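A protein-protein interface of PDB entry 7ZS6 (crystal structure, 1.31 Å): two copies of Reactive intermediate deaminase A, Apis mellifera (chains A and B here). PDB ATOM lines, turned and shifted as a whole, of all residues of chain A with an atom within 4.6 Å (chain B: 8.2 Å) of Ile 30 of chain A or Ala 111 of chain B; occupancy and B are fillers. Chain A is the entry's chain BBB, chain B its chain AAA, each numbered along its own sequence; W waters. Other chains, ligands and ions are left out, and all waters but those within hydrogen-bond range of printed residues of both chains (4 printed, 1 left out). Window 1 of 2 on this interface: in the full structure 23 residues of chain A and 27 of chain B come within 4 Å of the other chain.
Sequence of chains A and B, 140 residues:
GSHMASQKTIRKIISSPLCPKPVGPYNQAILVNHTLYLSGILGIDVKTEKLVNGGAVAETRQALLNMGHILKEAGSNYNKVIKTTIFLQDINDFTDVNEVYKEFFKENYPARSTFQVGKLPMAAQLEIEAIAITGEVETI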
ATOM      1  N   ARG A  11      37.776  31.679 -24.042  1.00  0.00           N
ATOM      2  CA  ARG A  11      36.676  30.720 -24.139  1.00  0.00           C
ATOM      3  C   ARG A  11      37.251  29.418 -24.641  1.00  0.00           C
ATOM      4  O   ARG A  11      37.970  29.395 -25.670  1.00  0.00           O
ATOM      5  CB  ARG A  11      35.625  31.236 -25.121  1.00  0.00           C
ATOM      6  CG  ARG A  11      34.576  30.185 -25.466  1.00  0.00           C
ATOM      7  CD  ARG A  11      33.389  30.765 -26.159  1.00  0.00           C
ATOM      8  NE  ARG A  11      33.737  31.366 -27.425  1.00  0.00           N
ATOM      9  CZ  ARG A  11      32.856  31.948 -28.222  1.00  0.00           C
ATOM     10  NH1 ARG A  11      31.567  31.944 -27.901  1.00  0.00           N
ATOM     11  NH2 ARG A  11      33.278  32.651 -29.251  1.00  0.00           N
ATOM     12  N   LYS A  12      36.855  28.328 -24.029  1.00  0.00           N
ATOM     13  CA  LYS A  12      37.153  27.005 -24.610  1.00  0.00           C
ATOM     14  C   LYS A  12      35.862  26.204 -24.789  1.00  0.00           C
ATOM     15  O   LYS A  12      34.986  26.189 -23.903  1.00  0.00           O
ATOM     16  CB  LYS A  12      38.115  26.172 -23.764  1.00  0.00           C
ATOM     17  CG  LYS A  12      38.526  24.873 -24.447  1.00  0.00           C
ATOM     18  CD  LYS A  12      39.395  23.935 -23.607  1.00  0.00           C
ATOM     19  CE  LYS A  12      39.560  22.562 -24.222  1.00  0.00           C
ATOM     20  NZ  LYS A  12      40.458  22.616 -25.392  1.00  0.00           N
ATOM     21  N   ILE A  13      35.720  25.616 -25.953  1.00  0.00           N
ATOM     22  CA  ILE A  13      34.603  24.703 -26.279  1.00  0.00           C
ATOM     23  C   ILE A  13      34.934  23.349 -25.674  1.00  0.00           C
ATOM     24  O   ILE A  13      35.983  22.763 -25.999  1.00  0.00           O
ATOM     25  CB  ILE A  13      34.414  24.618 -27.790  1.00  0.00           C
ATOM     26  CG1 ILE A  13      34.412  25.994 -28.475  1.00  0.00           C
ATOM     27  CG2 ILE A  13      33.260  23.736 -28.136  1.00  0.00           C
ATOM     28  CD1 ILE A  13      33.555  27.034 -27.915  1.00  0.00           C
ATOM     29  N   ASN A  27      26.882  23.241 -27.543  1.00  0.00           N
ATOM     30  CA  ASN A  27      28.072  22.540 -27.024  1.00  0.00           C
ATOM     31  C   ASN A  27      27.740  21.960 -25.651  1.00  0.00           C
ATOM     32  O   ASN A  27      26.953  22.532 -24.888  1.00  0.00           O
ATOM     33  CB  ASN A  27      29.280  23.449 -27.006  1.00  0.00           C
ATOM     34  CG  ASN A  27      29.920  23.443 -28.379  1.00  0.00           C
ATOM     35  OD1 ASN A  27      30.389  22.380 -28.823  1.00  0.00           O
ATOM     36  ND2 ASN A  27      29.880  24.578 -29.067  1.00  0.00           N
ATOM     37  N   ALA A  29      29.558  21.917 -23.063  1.00  0.00           N
ATOM     38  CA  ALA A  29      29.897  22.943 -22.096  1.00  0.00           C
ATOM     39  C   ALA A  29      30.772  23.989 -22.768  1.00  0.00           C
ATOM     40  O   ALA A  29      31.389  23.739 -23.801  1.00  0.00           O
ATOM     41  CB  ALA A  29      30.561  22.400 -20.855  1.00  0.00           C
ATOM     42  N   ILE A  30      30.724  25.178 -22.160  1.00  0.00           N
ATOM     43  CA  ILE A  30      31.554  26.311 -22.568  1.00  0.00           C
ATOM     44  C   ILE A  30      32.301  26.749 -21.318  1.00  0.00           C
ATOM     45  O   ILE A  30      31.730  27.059 -20.313  1.00  0.00           O
ATOM     46  CB  ILE A  30      30.718  27.452 -23.218  1.00  0.00           C
ATOM     47  CG1 ILE A  30      29.974  27.032 -24.472  1.00  0.00           C
ATOM     48  CG2 ILE A  30      31.616  28.643 -23.511  1.00  0.00           C
ATOM     49  CD1 ILE A  30      30.822  26.694 -25.666  1.00  0.00           C
ATOM     50  N   LEU A  31      33.618  26.892 -21.478  1.00  0.00           N
ATOM     51  CA  LEU A  31      34.497  27.397 -20.409  1.00  0.00           C
ATOM     52  C   LEU A  31      34.826  28.846 -20.721  1.00  0.00           C
ATOM     53  O   LEU A  31      35.267  29.089 -21.839  1.00  0.00           O
ATOM     54  CB  LEU A  31      35.759  26.502 -20.373  1.00  0.00           C
ATOM     55  CG  LEU A  31      36.745  26.884 -19.291  1.00  0.00           C
ATOM     56  CD1 LEU A  31      36.179  26.848 -17.882  1.00  0.00           C
ATOM     57  CD2 LEU A  31      37.968  26.021 -19.359  1.00  0.00           C
ATOM     58  N   VAL A  32      34.583  29.698 -19.759  1.00  0.00           N
ATOM     59  CA  VAL A  32      34.896  31.146 -19.826  1.00  0.00           C
ATOM     60  C   VAL A  32      35.863  31.441 -18.683  1.00  0.00           C
ATOM     61  O   VAL A  32      35.392  31.408 -17.559  1.00  0.00           O
ATOM     62  CB  VAL A  32      33.611  31.979 -19.661  1.00  0.00           C
ATOM     63  CG1 VAL A  32      33.951  33.453 -19.795  1.00  0.00           C
ATOM     64  CG2 VAL A  32      32.550  31.555 -20.653  1.00  0.00           C
ATOM     65  N   THR A  35      35.260  29.496 -15.374  1.00  0.00           N
ATOM     66  CA  THR A  35      33.840  29.153 -15.090  1.00  0.00           C
ATOM     67  C   THR A  35      33.264  28.338 -16.249  1.00  0.00           C
ATOM     68  O   THR A  35      33.279  28.731 -17.429  1.00  0.00           O
ATOM     69  CB  THR A  35      32.986  30.413 -14.893  1.00  0.00           C
ATOM     70  OG1 THR A  35      33.544  31.192 -13.842  1.00  0.00           O
ATOM     71  CG2 THR A  35      31.573  30.083 -14.483  1.00  0.00           C
ATOM     72  N   LEU A  36      32.819  27.139 -15.879  1.00  0.00           N
ATOM     73  CA  LEU A  36      32.345  26.130 -16.856  1.00  0.00           C
ATOM     74  C   LEU A  36      30.798  26.110 -16.816  1.00  0.00           C
ATOM     75  O   LEU A  36      30.228  25.823 -15.783  1.00  0.00           O
ATOM     76  CB  LEU A  36      32.907  24.776 -16.458  1.00  0.00           C
ATOM     77  CG  LEU A  36      32.559  23.687 -17.449  1.00  0.00           C
ATOM     78  CD1 LEU A  36      33.227  23.874 -18.825  1.00  0.00           C
ATOM     79  CD2 LEU A  36      32.965  22.357 -16.889  1.00  0.00           C
ATOM     80  N   TYR A  37      30.200  26.407 -17.957  1.00  0.00           N
ATOM     81  CA  TYR A  37      28.724  26.405 -18.099  1.00  0.00           C
ATOM     82  C   TYR A  37      28.350  25.118 -18.881  1.00  0.00           C
ATOM     83  O   TYR A  37      28.680  24.959 -20.054  1.00  0.00           O
ATOM     84  CB  TYR A  37      28.278  27.624 -18.887  1.00  0.00           C
ATOM     85  CG  TYR A  37      28.523  28.928 -18.210  1.00  0.00           C
ATOM     86  CD1 TYR A  37      29.744  29.579 -18.285  1.00  0.00           C
ATOM     87  CD2 TYR A  37      27.538  29.503 -17.427  1.00  0.00           C
ATOM     88  CE1 TYR A  37      29.938  30.788 -17.656  1.00  0.00           C
ATOM     89  CE2 TYR A  37      27.745  30.717 -16.767  1.00  0.00           C
ATOM     90  CZ  TYR A  37      28.985  31.327 -16.837  1.00  0.00           C
ATOM     91  OH  TYR A  37      29.171  32.553 -16.218  1.00  0.00           O
ATOM     92  N   LEU A  38      27.713  24.220 -18.167  1.00  0.00           N
ATOM     93  CA  LEU A  38      27.303  22.913 -18.720  1.00  0.00           C
ATOM     94  C   LEU A  38      25.883  23.008 -19.281  1.00  0.00           C
ATOM     95  O   LEU A  38      24.999  23.540 -18.611  1.00  0.00           O
ATOM     96  CB  LEU A  38      27.396  21.777 -17.734  1.00  0.00           C
ATOM     97  CG  LEU A  38      28.801  21.411 -17.233  1.00  0.00           C
ATOM     98  CD1 LEU A  38      29.270  22.281 -16.069  1.00  0.00           C
ATOM     99  CD2 LEU A  38      28.811  19.965 -16.777  1.00  0.00           C
ATOM    100  N   SER A  39      25.660  22.465 -20.444  1.00  0.00           N
ATOM    101  CA  SER A  39      24.315  22.205 -20.963  1.00  0.00           C
ATOM    102  C   SER A  39      23.570  21.269 -20.042  1.00  0.00           C
ATOM    103  O   SER A  39      24.148  20.420 -19.376  1.00  0.00           O
ATOM    104  CB  SER A  39      24.410  21.600 -22.296  1.00  0.00           C
ATOM    105  OG  SER A  39      24.880  22.537 -23.269  1.00  0.00           O
ATOM    106  N   LYS B  80      29.342  35.353 -29.258  1.00  0.00           N
ATOM    107  CA  LYS B  80      29.905  35.518 -27.913  1.00  0.00           C
ATOM    108  C   LYS B  80      28.861  35.112 -26.858  1.00  0.00           C
ATOM    109  O   LYS B  80      29.140  35.264 -25.706  1.00  0.00           O
ATOM    110  CB  LYS B  80      30.443  36.921 -27.702  1.00  0.00           C
ATOM    111  CG  LYS B  80      31.622  37.233 -28.617  1.00  0.00           C
ATOM    112  CD  LYS B  80      32.041  38.739 -28.493  1.00  0.00           C
ATOM    113  CE  LYS B  80      33.180  39.120 -29.421  1.00  0.00           C
ATOM    114  NZ  LYS B  80      33.561  40.552 -29.268  1.00  0.00           N
ATOM    115  N   VAL B  81      27.766  34.501 -27.279  1.00  0.00           N
ATOM    116  CA  VAL B  81      26.812  33.904 -26.315  1.00  0.00           C
ATOM    117  C   VAL B  81      27.388  32.597 -25.782  1.00  0.00           C
ATOM    118  O   VAL B  81      27.861  31.776 -26.585  1.00  0.00           O
ATOM    119  CB  VAL B  81      25.418  33.779 -26.939  1.00  0.00           C
ATOM    120  CG1 VAL B  81      24.469  33.023 -26.006  1.00  0.00           C
ATOM    121  CG2 VAL B  81      24.839  35.127 -27.298  1.00  0.00           C
ATOM    122  N   ILE B  82      27.355  32.447 -24.474  1.00  0.00           N
ATOM    123  CA  ILE B  82      27.962  31.356 -23.658  1.00  0.00           C
ATOM    124  C   ILE B  82      26.937  30.262 -23.390  1.00  0.00           C
ATOM    125  O   ILE B  82      27.283  29.108 -23.435  1.00  0.00           O
ATOM    126  CB  ILE B  82      28.505  31.903 -22.321  1.00  0.00           C
ATOM    127  CG1 ILE B  82      29.590  32.938 -22.604  1.00  0.00           C
ATOM    128  CG2 ILE B  82      28.982  30.764 -21.401  1.00  0.00           C
ATOM    129  CD1 ILE B  82      30.519  32.532 -23.805  1.00  0.00           C
ATOM    130  N   LYS B  83      25.742  30.681 -22.999  1.00  0.00           N
ATOM    131  CA  LYS B  83      24.713  29.737 -22.525  1.00  0.00           C
ATOM    132  C   LYS B  83      23.356  30.338 -22.830  1.00  0.00           C
ATOM    133  O   LYS B  83      23.156  31.538 -22.604  1.00  0.00           O
ATOM    134  CB  LYS B  83      24.884  29.462 -21.043  1.00  0.00           C
ATOM    135  CG  LYS B  83      23.730  28.781 -20.324  1.00  0.00           C
ATOM    136  CD  LYS B  83      23.899  27.354 -20.394  1.00  0.00           C
ATOM    137  CE  LYS B  83      22.905  26.484 -19.600  1.00  0.00           C
ATOM    138  NZ  LYS B  83      21.547  27.019 -19.613  1.00  0.00           N
ATOM    139  N   THR B  84      22.450  29.521 -23.343  1.00  0.00           N
ATOM    140  CA  THR B  84      21.035  29.897 -23.474  1.00  0.00           C
ATOM    141  C   THR B  84      20.176  28.898 -22.713  1.00  0.00           C
ATOM    142  O   THR B  84      20.532  27.716 -22.559  1.00  0.00           O
ATOM    143  CB  THR B  84      20.578  30.021 -24.910  1.00  0.00           C
ATOM    144  OG1 THR B  84      20.683  28.728 -25.510  1.00  0.00           O
ATOM    145  CG2 THR B  84      21.409  31.013 -25.702  1.00  0.00           C
ATOM    146  N   THR B  85      19.015  29.335 -22.264  1.00  0.00           N
ATOM    147  CA  THR B  85      17.940  28.495 -21.763  1.00  0.00           C
ATOM    148  C   THR B  85      16.698  28.793 -22.552  1.00  0.00           C
ATOM    149  O   THR B  85      16.345  29.975 -22.675  1.00  0.00           O
ATOM    150  CB  THR B  85      17.713  28.604 -20.285  1.00  0.00           C
ATOM    151  OG1 THR B  85      18.934  28.392 -19.606  1.00  0.00           O
ATOM    152  CG2 THR B  85      16.716  27.561 -19.828  1.00  0.00           C
ATOM    153  N   ILE B  86      16.121  27.792 -23.170  1.00  0.00           N
ATOM    154  CA  ILE B  86      14.904  27.929 -23.979  1.00  0.00           C
ATOM    155  C   ILE B  86      13.735  27.378 -23.179  1.00  0.00           C
ATOM    156  O   ILE B  86      13.715  26.183 -22.812  1.00  0.00           O
ATOM    157  CB  ILE B  86      15.052  27.211 -25.313  1.00  0.00           C
ATOM    158  CG1 ILE B  86      16.249  27.772 -26.108  1.00  0.00           C
ATOM    159  CG2 ILE B  86      13.763  27.281 -26.121  1.00  0.00           C
ATOM    160  CD1 ILE B  86      16.481  27.064 -27.439  1.00  0.00           C
ATOM    161  N   TYR B 101      16.859  28.867 -34.386  1.00  0.00           N
ATOM    162  CA  TYR B 101      18.039  29.122 -33.581  1.00  0.00           C
ATOM    163  C   TYR B 101      19.256  29.097 -34.483  1.00  0.00           C
ATOM    164  O   TYR B 101      20.170  29.928 -34.301  1.00  0.00           O
ATOM    165  CB  TYR B 101      18.065  28.085 -32.459  1.00  0.00           C
ATOM    166  CG  TYR B 101      19.055  28.312 -31.358  1.00  0.00           C
ATOM    167  CD1 TYR B 101      18.726  28.997 -30.200  1.00  0.00           C
ATOM    168  CD2 TYR B 101      20.317  27.725 -31.405  1.00  0.00           C
ATOM    169  CE1 TYR B 101      19.591  29.057 -29.117  1.00  0.00           C
ATOM    170  CE2 TYR B 101      21.198  27.807 -30.356  1.00  0.00           C
ATOM    171  CZ  TYR B 101      20.838  28.479 -29.213  1.00  0.00           C
ATOM    172  OH  TYR B 101      21.676  28.578 -28.145  1.00  0.00           O
ATOM    173  N   PHE B 105      22.794  31.375 -34.511  1.00  0.00           N
ATOM    174  CA  PHE B 105      23.996  30.774 -33.910  1.00  0.00           C
ATOM    175  C   PHE B 105      24.581  29.842 -34.958  1.00  0.00           C
ATOM    176  O   PHE B 105      23.940  28.873 -35.352  1.00  0.00           O
ATOM    177  CB  PHE B 105      23.613  30.086 -32.605  1.00  0.00           C
ATOM    178  CG  PHE B 105      23.021  31.015 -31.586  1.00  0.00           C
ATOM    179  CD1 PHE B 105      23.856  31.857 -30.875  1.00  0.00           C
ATOM    180  CD2 PHE B 105      21.685  31.077 -31.342  1.00  0.00           C
ATOM    181  CE1 PHE B 105      23.357  32.728 -29.957  1.00  0.00           C
ATOM    182  CE2 PHE B 105      21.177  31.988 -30.449  1.00  0.00           C
ATOM    183  CZ  PHE B 105      21.993  32.806 -29.735  1.00  0.00           C
ATOM    184  N   GLU B 107      28.390  29.223 -35.133  1.00  0.00           N
ATOM    185  CA  GLU B 107      29.705  28.700 -34.718  1.00  0.00           C
ATOM    186  C   GLU B 107      29.868  28.833 -33.217  1.00  0.00           C
ATOM    187  O   GLU B 107      29.165  29.601 -32.616  1.00  0.00           O
ATOM    188  CB  GLU B 107      30.828  29.473 -35.454  1.00  0.00           C
ATOM    189  CG  GLU B 107      30.965  30.915 -34.910  1.00  0.00           C
ATOM    190  CD  GLU B 107      31.587  31.984 -35.794  1.00  0.00           C
ATOM    191  OE1 GLU B 107      31.291  31.973 -37.002  1.00  0.00           O
ATOM    192  OE2 GLU B 107      32.345  32.848 -35.264  1.00  0.00           O
ATOM    193  N   ASN B 108      30.789  28.058 -32.628  1.00  0.00           N
ATOM    194  CA  ASN B 108      31.160  28.231 -31.201  1.00  0.00           C
ATOM    195  C   ASN B 108      29.848  28.226 -30.417  1.00  0.00           C
ATOM    196  O   ASN B 108      29.645  29.096 -29.544  1.00  0.00           O
ATOM    197  CB  ASN B 108      32.017  29.459 -30.897  1.00  0.00           C
ATOM    198  CG  ASN B 108      33.405  29.311 -31.490  1.00  0.00           C
ATOM    199  OD1 ASN B 108      33.969  28.249 -31.491  1.00  0.00           O
ATOM    200  ND2 ASN B 108      33.925  30.343 -32.084  1.00  0.00           N
ATOM    201  N   TYR B 109      29.000  27.231 -30.681  1.00  0.00           N
ATOM    202  CA  TYR B 109      27.615  27.290 -30.209  1.00  0.00           C
ATOM    203  C   TYR B 109      27.578  27.374 -28.692  1.00  0.00           C
ATOM    204  O   TYR B 109      28.338  26.732 -27.949  1.00  0.00           O
ATOM    205  CB  TYR B 109      26.841  26.054 -30.612  1.00  0.00           C
ATOM    206  CG  TYR B 109      26.813  25.765 -32.072  1.00  0.00           C
ATOM    207  CD1 TYR B 109      25.986  26.520 -32.888  1.00  0.00           C
ATOM    208  CD2 TYR B 109      27.592  24.753 -32.624  1.00  0.00           C
ATOM    209  CE1 TYR B 109      25.911  26.273 -34.251  1.00  0.00           C
ATOM    210  CE2 TYR B 109      27.521  24.494 -33.984  1.00  0.00           C
ATOM    211  CZ  TYR B 109      26.682  25.265 -34.783  1.00  0.00           C
ATOM    212  OH  TYR B 109      26.594  25.032 -36.113  1.00  0.00           O
ATOM    213  N   PRO B 110      26.593  28.119 -28.145  1.00  0.00           N
ATOM    214  CA  PRO B 110      26.403  28.137 -26.703  1.00  0.00           C
ATOM    215  C   PRO B 110      26.100  26.783 -26.084  1.00  0.00           C
ATOM    216  O   PRO B 110      25.542  25.935 -26.747  1.00  0.00           O
ATOM    217  CB  PRO B 110      25.190  29.066 -26.522  1.00  0.00           C
ATOM    218  CG  PRO B 110      25.165  29.889 -27.753  1.00  0.00           C
ATOM    219  CD  PRO B 110      25.698  29.006 -28.875  1.00  0.00           C
ATOM    220  N   ALA B 111      26.392  26.686 -24.814  1.00  0.00           N
ATOM    221  CA  ALA B 111      25.750  25.642 -23.999  1.00  0.00           C
ATOM    222  C   ALA B 111      24.242  25.900 -24.007  1.00  0.00           C
ATOM    223  O   ALA B 111      23.853  27.094 -24.206  1.00  0.00           O
ATOM    224  CB  ALA B 111      26.307  25.624 -22.628  1.00  0.00           C
ATOM    225  N   ARG B 112      23.423  24.935 -23.700  1.00  0.00           N
ATOM    226  CA  ARG B 112      21.966  25.137 -23.844  1.00  0.00           C
ATOM    227  C   ARG B 112      21.238  24.193 -22.915  1.00  0.00           C
ATOM    228  O   ARG B 112      21.639  23.031 -22.734  1.00  0.00           O
ATOM    229  CB  ARG B 112      21.561  24.894 -25.307  1.00  0.00           C
ATOM    230  CG  ARG B 112      20.144  25.347 -25.605  1.00  0.00           C
ATOM    231  CD  ARG B 112      19.868  25.455 -27.076  1.00  0.00           C
ATOM    232  NE  ARG B 112      19.831  24.112 -27.657  1.00  0.00           N
ATOM    233  CZ  ARG B 112      19.456  23.820 -28.929  1.00  0.00           C
ATOM    234  NH1 ARG B 112      19.094  24.838 -29.770  1.00  0.00           N
ATOM    235  NH2 ARG B 112      19.485  22.518 -29.315  1.00  0.00           N
ATOM    236  N   SER B 113      20.092  24.640 -22.402  1.00  0.00           N
ATOM    237  CA  SER B 113      19.097  23.778 -21.787  1.00  0.00           C
ATOM    238  C   SER B 113      17.734  24.182 -22.305  1.00  0.00           C
ATOM    239  O   SER B 113      17.543  25.336 -22.646  1.00  0.00           O
ATOM    240  CB  SER B 113      19.083  23.984 -20.314  1.00  0.00           C
ATOM    241  OG  SER B 113      20.315  23.574 -19.741  1.00  0.00           O
ATOM    242  N   THR B 114      16.847  23.219 -22.441  1.00  0.00           N
ATOM    243  CA  THR B 114      15.534  23.427 -23.000  1.00  0.00           C
ATOM    244  C   THR B 114      14.513  22.614 -22.237  1.00  0.00           C
ATOM    245  O   THR B 114      14.758  21.445 -21.916  1.00  0.00           O
ATOM    246  CB  THR B 114      15.474  23.032 -24.472  1.00  0.00           C
ATOM    247  OG1 THR B 114      16.485  23.711 -25.227  1.00  0.00           O
ATOM    248  CG2 THR B 114      14.118  23.362 -25.090  1.00  0.00           C
ATOM    249  N   GLU B 129      16.488  32.942 -22.358  1.00  0.00           N
ATOM    250  CA  GLU B 129      17.438  33.743 -21.553  1.00  0.00           C
ATOM    251  C   GLU B 129      18.846  33.338 -21.936  1.00  0.00           C
ATOM    252  O   GLU B 129      19.093  32.267 -22.417  1.00  0.00           O
ATOM    253  CB  GLU B 129      17.263  33.696 -20.036  1.00  0.00           C
ATOM    254  CG  GLU B 129      17.526  32.337 -19.444  1.00  0.00           C
ATOM    255  CD  GLU B 129      17.303  32.262 -17.953  1.00  0.00           C
ATOM    256  OE1 GLU B 129      16.815  33.236 -17.366  1.00  0.00           O
ATOM    257  OE2 GLU B 129      17.649  31.259 -17.415  1.00  0.00           O
ATOM    258  N   ALA B 130      19.782  34.228 -21.762  1.00  0.00           N
ATOM    259  CA  ALA B 130      21.148  33.972 -22.190  1.00  0.00           C
ATOM    260  C   ALA B 130      22.142  34.650 -21.289  1.00  0.00           C
ATOM    261  O   ALA B 130      21.820  35.589 -20.585  1.00  0.00           O
ATOM    262  CB  ALA B 130      21.350  34.467 -23.598  1.00  0.00           C
ATOM    263  N   ILE B 131      23.362  34.144 -21.374  1.00  0.00           N
ATOM    264  CA  ILE B 131      24.585  34.728 -20.800  1.00  0.00           C
ATOM    265  C   ILE B 131      25.579  34.867 -21.946  1.00  0.00           C
ATOM    266  O   ILE B 131      25.679  33.953 -22.768  1.00  0.00           O
ATOM    267  CB  ILE B 131      25.163  33.869 -19.670  1.00  0.00           C
ATOM    268  CG1 ILE B 131      24.133  33.733 -18.539  1.00  0.00           C
ATOM    269  CG2 ILE B 131      26.462  34.459 -19.171  1.00  0.00           C
ATOM    270  CD1 ILE B 131      24.511  32.761 -17.462  1.00  0.00           C
ATOM    271  N   ILE B 133      29.396  37.105 -23.437  1.00  0.00           N
ATOM    272  CA  ILE B 133      30.688  37.787 -23.109  1.00  0.00           C
ATOM    273  C   ILE B 133      30.794  39.056 -23.946  1.00  0.00           C
ATOM    274  O   ILE B 133      30.429  39.033 -25.117  1.00  0.00           O
ATOM    275  CB  ILE B 133      31.891  36.890 -23.437  1.00  0.00           C
ATOM    276  CG1 ILE B 133      31.847  35.630 -22.598  1.00  0.00           C
ATOM    277  CG2 ILE B 133      33.223  37.590 -23.258  1.00  0.00           C
ATOM    278  CD1 ILE B 133      31.689  35.926 -21.149  1.00  0.00           C
ATOM    279  N   VAL B 137      37.386  38.142 -27.247  1.00  0.00           N
ATOM    280  CA  VAL B 137      37.297  36.712 -26.867  1.00  0.00           C
ATOM    281  C   VAL B 137      38.254  35.932 -27.721  1.00  0.00           C
ATOM    282  O   VAL B 137      38.025  35.909 -28.944  1.00  0.00           O
ATOM    283  CB  VAL B 137      35.869  36.172 -27.053  1.00  0.00           C
ATOM    284  CG1 VAL B 137      35.759  34.696 -26.662  1.00  0.00           C
ATOM    285  CG2 VAL B 137      34.926  37.058 -26.241  1.00  0.00           C
ATOM    286  N   THR B 139      39.067  32.165 -28.609  1.00  0.00           N
ATOM    287  CA  THR B 139      38.463  30.828 -28.504  1.00  0.00           C
ATOM    288  C   THR B 139      39.482  29.735 -28.841  1.00  0.00           C
ATOM    289  O   THR B 139      40.023  29.782 -29.927  1.00  0.00           O
ATOM    290  CB  THR B 139      37.199  30.735 -29.355  1.00  0.00           C
ATOM    291  OG1 THR B 139      36.313  31.713 -28.780  1.00  0.00           O
ATOM    292  CG2 THR B 139      36.640  29.333 -29.288  1.00  0.00           C
ATOM    293  N   ILE B 140      39.624  28.769 -27.936  1.00  0.00           N
ATOM    294  CA  ILE B 140      40.348  27.472 -28.099  1.00  0.00           C
ATOM    295  C   ILE B 140      39.398  26.264 -27.840  1.00  0.00           C
ATOM    296  O   ILE B 140      39.981  25.151 -27.775  1.00  0.00           O
ATOM    297  CB  ILE B 140      41.561  27.521 -27.150  1.00  0.00           C
ATOM    298  CG1 ILE B 140      41.165  27.459 -25.672  1.00  0.00           C
ATOM    299  CG2 ILE B 140      42.365  28.776 -27.407  1.00  0.00           C
ATOM    300  CD1 ILE B 140      42.258  27.786 -24.685  1.00  0.00           C
ATOM    301  OXT ILE B 140      38.063  26.175 -27.680  1.00  0.00           O
HETATM  302  O   HOH W   1      29.922  29.902 -26.738  1.00  0.00           O
HETATM  303  O   HOH W   2      28.508  31.716 -29.248  1.00  0.00           O
HETATM  304  O   HOH W   3      36.171  33.843 -30.182  1.00  0.00           O
HETATM  305  O   HOH W   4      38.106  23.119 -27.613  1.00  0.00           O
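Of the 13 printed residues of chain A, 9 touch a printed residue of chain B.
Printed residues of chain A that touch a printed residue of chain B: Arg 11, Lys 12, Ile 13, Asn 27, Ile 30, Val 32, Tyr 37, Leu 38 and Ser 39.
Hydrophobic or aromatic side chains of chain A within 4 Å of the printed part of chain B: Ile 13, Ile 30, Val 32 and Tyr 37.
Hydrophobic or aromatic side chains of chain B that line the printed part of chain A: Ile 82, Tyr 109, Ala 111, Ile 131, Ile 133, Val 137 and Ile 140.
Among the printed residues, no Asp or Glu carboxylate lies within 4 Å of a Lys or Arg side-chain nitrogen of the other chain.
Printed residues of chain B within 4 Å of Ile 30 of chain A: Ile 82, Tyr 109 and Ala 111.
Of the printed residues of chain A, Val 81 of chain B touches Arg 11.
Glu 107 of chain B touches none of the printed residues of chain A.
Ala 111 of chain B touches just these residues of chain A: Asn 27, Ile 30, Tyr 37 and Ser 39.
Of the printed residues of chain A, Thr 139 of chain B touches Arg 11 (2.9 Å).
The nearest printed residue of chain B that does not touch Ile 30 of chain A is Pro 110 of chain B (4.2 Å).
The nearest printed residue of chain B that does not touch Arg 11 of chain A is Ile 82 of chain B (4.1 Å).
O of Ile 140 of chain B lies within salt-bridge range of NZ of Lys 12 of chain A (3.5 Å).
OXT of Ile 140 of chain B is in hydrogen-bond range of N of Ile 13 of chain A, at 3.0 Å.
ND2 of Asn 27 of chain A lies within hydrogen-bond range of O of Tyr 109 of chain B, 2.9 Å away.
The backbone carbonyl oxygen (O) of Pro 110 of chain B is in hydrogen-bond range of the backbone NH (N) of Asn 27 of chain A (3.1 Å).
NE of Arg 11 of chain A is in hydrogen-bond range of OG1 of Thr 139 of chain B.
OG of Ser 39 of chain A lies within hydrogen-bond range of N of Arg 112 of chain B, 2.8 Å away.
The backbone carbonyl oxygen of Arg 11 of chain A lies within hydrogen-bond range of the backbone NH of Ile 140 of chain B (2.9 Å).
ND2 of Asn 108 of chain B touches NH2 of Arg 11 of chain A, 3.7 Å away.
CB of Arg 11 of chain A touches CG1 of Val 137 of chain B, 3.8 Å away.
CD1 of Ile 30 of chain A touches O of Tyr 109 of chain B, at 3.4 Å.
Ile 133 of chain B touches Val 32 of chain A.
Lys 83 of chain B touches Leu 38 of chain A (CE to O, 3.7 Å).
Water W1 lies within hydrogen-bond range of O of Val 81 of chain B (2.8 Å), NH1 of Arg 11 of chain A (2.9 Å) and O of Asn 108 of chain B (2.9 Å).
The backbone carbonyl oxygen (O) of Asn 27 of chain A lies within hydrogen-bond range of the side-chain hydroxyl (OG) of Ser 39 of chain A (2.6 Å).
NZ of Lys 83 of chain B sits at hydrogen-bond distance from OG1 of Thr 85 of chain B, at 3.0 Å.
No position is printed for both chains.
Of the 25 pairs that touch across the chains among the printed residues, none has its exchanged pair printed and touching as well.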
